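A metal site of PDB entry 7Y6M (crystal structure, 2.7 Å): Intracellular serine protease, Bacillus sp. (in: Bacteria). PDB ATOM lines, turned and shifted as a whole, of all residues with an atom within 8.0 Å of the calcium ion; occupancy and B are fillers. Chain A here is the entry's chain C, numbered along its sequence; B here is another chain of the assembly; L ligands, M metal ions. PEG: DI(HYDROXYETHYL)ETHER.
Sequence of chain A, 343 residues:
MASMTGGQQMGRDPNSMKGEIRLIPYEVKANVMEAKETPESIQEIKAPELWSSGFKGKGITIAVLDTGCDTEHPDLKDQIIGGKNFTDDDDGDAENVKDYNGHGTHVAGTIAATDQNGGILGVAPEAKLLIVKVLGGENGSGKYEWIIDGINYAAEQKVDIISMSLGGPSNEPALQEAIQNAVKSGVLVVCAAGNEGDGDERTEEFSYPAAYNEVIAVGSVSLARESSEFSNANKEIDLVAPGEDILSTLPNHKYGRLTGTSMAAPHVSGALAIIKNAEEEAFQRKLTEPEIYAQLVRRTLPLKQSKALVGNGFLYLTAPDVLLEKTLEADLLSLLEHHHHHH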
ATOM      1  N   VAL A 189     -24.837 -19.664  12.675  1.00  0.00           N
ATOM      2  CA  VAL A 189     -24.812 -20.328  11.371  1.00  0.00           C
ATOM      3  C   VAL A 189     -23.365 -20.411  10.878  1.00  0.00           C
ATOM      4  O   VAL A 189     -22.780 -19.406  10.463  1.00  0.00           O
ATOM      5  CB  VAL A 189     -25.703 -19.575  10.388  1.00  0.00           C
ATOM      6  CG1 VAL A 189     -25.631 -20.211   9.020  1.00  0.00           C
ATOM      7  CG2 VAL A 189     -27.128 -19.572  10.925  1.00  0.00           C
ATOM      8  N   PRO A 209     -23.231 -20.614   1.243  1.00  0.00           N
ATOM      9  CA  PRO A 209     -23.575 -19.418   2.021  1.00  0.00           C
ATOM     10  C   PRO A 209     -22.449 -18.715   2.778  1.00  0.00           C
ATOM     11  O   PRO A 209     -22.700 -17.612   3.260  1.00  0.00           O
ATOM     12  CB  PRO A 209     -24.605 -19.947   3.002  1.00  0.00           C
ATOM     13  CG  PRO A 209     -24.237 -21.351   3.214  1.00  0.00           C
ATOM     14  CD  PRO A 209     -23.709 -21.844   1.905  1.00  0.00           C
ATOM     15  N   ALA A 210     -21.254 -19.314   2.858  1.00  0.00           N
ATOM     16  CA  ALA A 210     -20.130 -18.714   3.595  1.00  0.00           C
ATOM     17  C   ALA A 210     -19.949 -17.214   3.347  1.00  0.00           C
ATOM     18  O   ALA A 210     -19.749 -16.428   4.276  1.00  0.00           O
ATOM     19  CB  ALA A 210     -18.840 -19.433   3.225  1.00  0.00           C
ATOM     20  N   ALA A 211     -20.015 -16.790   2.085  1.00  0.00           N
ATOM     21  CA  ALA A 211     -19.742 -15.409   1.734  1.00  0.00           C
ATOM     22  C   ALA A 211     -20.722 -14.393   2.352  1.00  0.00           C
ATOM     23  O   ALA A 211     -20.459 -13.187   2.259  1.00  0.00           O
ATOM     24  CB  ALA A 211     -19.740 -15.290   0.197  1.00  0.00           C
ATOM     25  N   TYR A 212     -21.829 -14.835   2.955  1.00  0.00           N
ATOM     26  CA  TYR A 212     -22.756 -13.875   3.547  1.00  0.00           C
ATOM     27  C   TYR A 212     -22.227 -13.400   4.892  1.00  0.00           C
ATOM     28  O   TYR A 212     -21.771 -14.196   5.707  1.00  0.00           O
ATOM     29  CB  TYR A 212     -24.131 -14.504   3.756  1.00  0.00           C
ATOM     30  CG  TYR A 212     -24.881 -14.867   2.505  1.00  0.00           C
ATOM     31  CD1 TYR A 212     -25.141 -13.915   1.534  1.00  0.00           C
ATOM     32  CD2 TYR A 212     -25.342 -16.164   2.307  1.00  0.00           C
ATOM     33  CE1 TYR A 212     -25.812 -14.252   0.395  1.00  0.00           C
ATOM     34  CE2 TYR A 212     -26.018 -16.501   1.181  1.00  0.00           C
ATOM     35  CZ  TYR A 212     -26.268 -15.546   0.230  1.00  0.00           C
ATOM     36  OH  TYR A 212     -26.960 -15.900  -0.895  1.00  0.00           O
ATOM     37  N   ASN A 213     -22.312 -12.080   5.116  1.00  0.00           N
ATOM     38  CA  ASN A 213     -21.649 -11.545   6.298  1.00  0.00           C
ATOM     39  C   ASN A 213     -22.119 -12.257   7.562  1.00  0.00           C
ATOM     40  O   ASN A 213     -21.316 -12.481   8.466  1.00  0.00           O
ATOM     41  CB  ASN A 213     -21.863 -10.044   6.426  1.00  0.00           C
ATOM     42  CG  ASN A 213     -21.159  -9.467   7.651  1.00  0.00           C
ATOM     43  OD1 ASN A 213     -21.708  -9.464   8.747  1.00  0.00           O
ATOM     44  ND2 ASN A 213     -19.936  -9.007   7.477  1.00  0.00           N
ATOM     45  N   GLU A 214     -23.387 -12.671   7.634  1.00  0.00           N
ATOM     46  CA  GLU A 214     -23.873 -13.246   8.881  1.00  0.00           C
ATOM     47  C   GLU A 214     -23.201 -14.582   9.206  1.00  0.00           C
ATOM     48  O   GLU A 214     -23.050 -14.923  10.385  1.00  0.00           O
ATOM     49  CB  GLU A 214     -25.386 -13.457   8.839  1.00  0.00           C
ATOM     50  CG  GLU A 214     -26.165 -12.306   8.330  1.00  0.00           C
ATOM     51  CD  GLU A 214     -26.596 -12.532   6.906  1.00  0.00           C
ATOM     52  OE1 GLU A 214     -27.732 -13.022   6.685  1.00  0.00           O
ATOM     53  OE2 GLU A 214     -25.771 -12.206   6.013  1.00  0.00           O
ATOM     54  N   VAL A 215     -22.843 -15.361   8.188  1.00  0.00           N
ATOM     55  CA  VAL A 215     -22.328 -16.694   8.437  1.00  0.00           C
ATOM     56  C   VAL A 215     -21.015 -16.602   9.190  1.00  0.00           C
ATOM     57  O   VAL A 215     -20.263 -15.631   9.047  1.00  0.00           O
ATOM     58  CB  VAL A 215     -22.157 -17.446   7.108  1.00  0.00           C
ATOM     59  CG1 VAL A 215     -21.737 -18.861   7.342  1.00  0.00           C
ATOM     60  CG2 VAL A 215     -23.460 -17.394   6.319  1.00  0.00           C
ATOM     61  N   ILE A 216     -20.735 -17.582  10.044  1.00  0.00           N
ATOM     62  CA  ILE A 216     -19.390 -17.740  10.585  1.00  0.00           C
ATOM     63  C   ILE A 216     -18.639 -18.590   9.559  1.00  0.00           C
ATOM     64  O   ILE A 216     -18.631 -19.817   9.614  1.00  0.00           O
ATOM     65  CB  ILE A 216     -19.378 -18.345  11.987  1.00  0.00           C
ATOM     66  CG1 ILE A 216     -20.450 -17.658  12.867  1.00  0.00           C
ATOM     67  CG2 ILE A 216     -18.010 -18.185  12.619  1.00  0.00           C
ATOM     68  CD1 ILE A 216     -20.355 -17.963  14.355  1.00  0.00           C
ATOM     69  N   ALA A 217     -18.018 -17.913   8.606  1.00  0.00           N
ATOM     70  CA  ALA A 217     -17.267 -18.572   7.541  1.00  0.00           C
ATOM     71  C   ALA A 217     -15.907 -19.023   8.061  1.00  0.00           C
ATOM     72  O   ALA A 217     -15.136 -18.218   8.591  1.00  0.00           O
ATOM     73  CB  ALA A 217     -17.081 -17.628   6.363  1.00  0.00           C
ATOM     74  N   VAL A 218     -15.613 -20.311   7.860  1.00  0.00           N
ATOM     75  CA  VAL A 218     -14.434 -20.945   8.433  1.00  0.00           C
ATOM     76  C   VAL A 218     -13.516 -21.394   7.318  1.00  0.00           C
ATOM     77  O   VAL A 218     -13.870 -22.272   6.527  1.00  0.00           O
ATOM     78  CB  VAL A 218     -14.801 -22.131   9.345  1.00  0.00           C
ATOM     79  CG1 VAL A 218     -13.560 -22.650  10.043  1.00  0.00           C
ATOM     80  CG2 VAL A 218     -15.883 -21.715  10.365  1.00  0.00           C
ATOM     81  N   LYS A 235     -13.375 -11.196   1.873  1.00  0.00           N
ATOM     82  CA  LYS A 235     -13.419 -10.303   3.024  1.00  0.00           C
ATOM     83  C   LYS A 235     -14.432 -10.750   4.047  1.00  0.00           C
ATOM     84  O   LYS A 235     -14.810  -9.955   4.909  1.00  0.00           O
ATOM     85  CB  LYS A 235     -13.707  -8.870   2.569  1.00  0.00           C
ATOM     86  CG  LYS A 235     -12.650  -8.297   1.648  1.00  0.00           C
ATOM     87  CD  LYS A 235     -12.663  -6.768   1.657  1.00  0.00           C
ATOM     88  CE  LYS A 235     -11.521  -6.186   0.819  1.00  0.00           C
ATOM     89  NZ  LYS A 235     -11.824  -6.060  -0.651  1.00  0.00           N
ATOM     90  N   GLU A 236     -14.901 -11.988   3.948  1.00  0.00           N
ATOM     91  CA  GLU A 236     -15.941 -12.505   4.825  1.00  0.00           C
ATOM     92  C   GLU A 236     -15.493 -13.749   5.580  1.00  0.00           C
ATOM     93  O   GLU A 236     -16.324 -14.457   6.178  1.00  0.00           O
ATOM     94  CB  GLU A 236     -17.209 -12.774   4.023  1.00  0.00           C
ATOM     95  CG  GLU A 236     -17.782 -11.558   3.359  1.00  0.00           C
ATOM     96  CD  GLU A 236     -18.154 -10.502   4.358  1.00  0.00           C
ATOM     97  OE1 GLU A 236     -18.484 -10.906   5.502  1.00  0.00           O
ATOM     98  OE2 GLU A 236     -18.110  -9.280   4.016  1.00  0.00           O
ATOM     99  N   ILE A 237     -14.200 -14.044   5.576  1.00  0.00           N
ATOM    100  CA  ILE A 237     -13.627 -15.053   6.449  1.00  0.00           C
ATOM    101  C   ILE A 237     -13.681 -14.544   7.881  1.00  0.00           C
ATOM    102  O   ILE A 237     -13.260 -13.422   8.171  1.00  0.00           O
ATOM    103  CB  ILE A 237     -12.189 -15.379   6.005  1.00  0.00           C
ATOM    104  CG1 ILE A 237     -12.135 -15.540   4.494  1.00  0.00           C
ATOM    105  CG2 ILE A 237     -11.637 -16.630   6.720  1.00  0.00           C
ATOM    106  CD1 ILE A 237     -13.023 -16.665   3.939  1.00  0.00           C
ATOM    107  N   ASP A 238     -14.203 -15.375   8.794  1.00  0.00           N
ATOM    108  CA  ASP A 238     -14.232 -15.000  10.208  1.00  0.00           C
ATOM    109  C   ASP A 238     -13.028 -15.549  10.965  1.00  0.00           C
ATOM    110  O   ASP A 238     -12.381 -14.825  11.747  1.00  0.00           O
ATOM    111  CB  ASP A 238     -15.513 -15.510  10.865  1.00  0.00           C
ATOM    112  CG  ASP A 238     -16.766 -14.962  10.202  1.00  0.00           C
ATOM    113  OD1 ASP A 238     -17.222 -13.908  10.632  1.00  0.00           O
ATOM    114  OD2 ASP A 238     -17.302 -15.611   9.272  1.00  0.00           O
ATOM    115  N   LEU A 239     -12.724 -16.834  10.784  1.00  0.00           N
ATOM    116  CA  LEU A 239     -11.601 -17.488  11.448  1.00  0.00           C
ATOM    117  C   LEU A 239     -11.273 -18.743  10.669  1.00  0.00           C
ATOM    118  O   LEU A 239     -11.974 -19.107   9.732  1.00  0.00           O
ATOM    119  CB  LEU A 239     -11.910 -17.800  12.914  1.00  0.00           C
ATOM    120  CG  LEU A 239     -12.823 -19.017  13.170  1.00  0.00           C
ATOM    121  CD1 LEU A 239     -12.956 -19.297  14.660  1.00  0.00           C
ATOM    122  CD2 LEU A 239     -14.203 -18.851  12.545  1.00  0.00           C
ATOM    123  N   TYR A 293     -20.606 -14.910  19.275  1.00  0.00           N
ATOM    124  CA  TYR A 293     -19.670 -14.638  18.181  1.00  0.00           C
ATOM    125  C   TYR A 293     -18.457 -13.863  18.686  1.00  0.00           C
ATOM    126  O   TYR A 293     -17.306 -14.258  18.446  1.00  0.00           O
ATOM    127  CB  TYR A 293     -20.367 -13.869  17.044  1.00  0.00           C
ATOM    128  CG  TYR A 293     -19.410 -13.421  15.942  1.00  0.00           C
ATOM    129  CD1 TYR A 293     -18.774 -14.353  15.109  1.00  0.00           C
ATOM    130  CD2 TYR A 293     -19.115 -12.075  15.738  1.00  0.00           C
ATOM    131  CE1 TYR A 293     -17.891 -13.961  14.105  1.00  0.00           C
ATOM    132  CE2 TYR A 293     -18.238 -11.673  14.739  1.00  0.00           C
ATOM    133  CZ  TYR A 293     -17.629 -12.622  13.933  1.00  0.00           C
ATOM    134  OH  TYR A 293     -16.754 -12.240  12.939  1.00  0.00           O
ATOM    135  N   ASN A 312      -9.981 -13.789  11.552  1.00  0.00           N
ATOM    136  CA  ASN A 312      -9.452 -13.285  12.805  1.00  0.00           C
ATOM    137  C   ASN A 312      -8.235 -14.070  13.250  1.00  0.00           C
ATOM    138  O   ASN A 312      -7.381 -13.535  13.975  1.00  0.00           O
ATOM    139  CB  ASN A 312     -10.525 -13.356  13.879  1.00  0.00           C
ATOM    140  CG  ASN A 312     -11.474 -12.182  13.837  1.00  0.00           C
ATOM    141  OD1 ASN A 312     -11.147 -11.096  14.316  1.00  0.00           O
ATOM    142  ND2 ASN A 312     -12.658 -12.389  13.290  1.00  0.00           N
ATOM    143  N   ARG B 285     -12.578  -3.483   4.633  1.00  0.00           N
ATOM    144  CA  ARG B 285     -13.980  -3.215   4.358  1.00  0.00           C
ATOM    145  C   ARG B 285     -14.538  -2.476   5.557  1.00  0.00           C
ATOM    146  O   ARG B 285     -13.804  -2.167   6.498  1.00  0.00           O
ATOM    147  CB  ARG B 285     -14.771  -4.498   4.063  1.00  0.00           C
ATOM    148  CG  ARG B 285     -14.717  -5.641   5.114  1.00  0.00           C
ATOM    149  CD  ARG B 285     -15.938  -6.561   4.931  1.00  0.00           C
ATOM    150  NE  ARG B 285     -15.929  -7.796   5.704  1.00  0.00           N
ATOM    151  CZ  ARG B 285     -16.511  -7.951   6.896  1.00  0.00           C
ATOM    152  NH1 ARG B 285     -17.125  -6.916   7.487  1.00  0.00           N
ATOM    153  NH2 ARG B 285     -16.461  -9.131   7.526  1.00  0.00           N
ATOM    154  N   THR B 288     -19.643  -4.418  10.511  1.00  0.00           N
ATOM    155  CA  THR B 288     -20.981  -4.263  11.053  1.00  0.00           C
ATOM    156  C   THR B 288     -20.920  -4.111  12.575  1.00  0.00           C
ATOM    157  O   THR B 288     -19.884  -4.333  13.218  1.00  0.00           O
ATOM    158  CB  THR B 288     -21.883  -5.451  10.683  1.00  0.00           C
ATOM    159  OG1 THR B 288     -21.706  -6.490  11.645  1.00  0.00           O
ATOM    160  CG2 THR B 288     -21.512  -5.985   9.372  1.00  0.00           C
ATOM    161  N   GLU B 291     -19.811  -7.211  14.371  1.00  0.00           N
ATOM    162  CA  GLU B 291     -18.377  -7.428  14.207  1.00  0.00           C
ATOM    163  C   GLU B 291     -17.567  -6.462  15.061  1.00  0.00           C
ATOM    164  O   GLU B 291     -16.567  -6.871  15.681  1.00  0.00           O
ATOM    165  CB  GLU B 291     -17.967  -7.260  12.748  1.00  0.00           C
ATOM    166  CG  GLU B 291     -18.530  -8.228  11.793  1.00  0.00           C
ATOM    167  CD  GLU B 291     -18.174  -7.816  10.398  1.00  0.00           C
ATOM    168  OE1 GLU B 291     -17.533  -8.622   9.680  1.00  0.00           O
ATOM    169  OE2 GLU B 291     -18.491  -6.668  10.020  1.00  0.00           O
HETATM  170  C1  PEG L   1     -21.270 -12.272  12.994  1.00  0.00           C
HETATM  171  O1  PEG L   1     -22.678 -12.235  13.270  1.00  0.00           O
HETATM  172  C2  PEG L   1     -20.921 -13.539  12.015  1.00  0.00           C
HETATM  173  O2  PEG L   1     -19.828 -13.214  11.092  1.00  0.00           O
HETATM  174  C3  PEG L   1     -19.727 -11.768  10.823  1.00  0.00           C
HETATM  175  C4  PEG L   1     -18.336 -11.353  10.241  1.00  0.00           C
HETATM  176  O4  PEG L   1     -18.226 -11.571   8.814  1.00  0.00           O
HETATM  177 CA    CA M   1     -19.067 -13.547   8.917  1.00  0.00          CA
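The side-chain amide nitrogen of Asn 213 sits at hydrogen-bond distance from the side-chain carboxylate of Glu 236, 3.1 Å away.
The side-chain carboxylate (OD1) of Asp 238 lies close to the side-chain hydroxyl (OH) of Tyr 293, at 2.9 Å.
NE of Arg 285 of chain B lies within salt-bridge range of OE2 of Glu 236 (3.1 Å).
The backbone carbonyl oxygen (O) of Asp 238 is in hydrogen-bond range of the backbone NH (N) of Asn 312, 2.6 Å away.
NH2 of Arg 285 of chain B sits close to ND2 of Asn 213 (3.5 Å).
N of Asp 238 sits at hydrogen-bond distance from O of Ala 217 (3.0 Å).
ND2 of Asn 213 is in hydrogen-bond range of OE1 of Glu 291 of chain B (3.3 Å).
O of Glu 236 touches the calcium ion, at 3.98 Å.
The calcium ion is bound by O4 of the ligand (2.1 Å), O2 of the ligand (2.3 Å), O of Val 215 (2.4 Å), O of Asn 213 (2.5 Å), OD1 of Asp 238 (2.5 Å) and OD2 of Asp 238 (2.7 Å).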
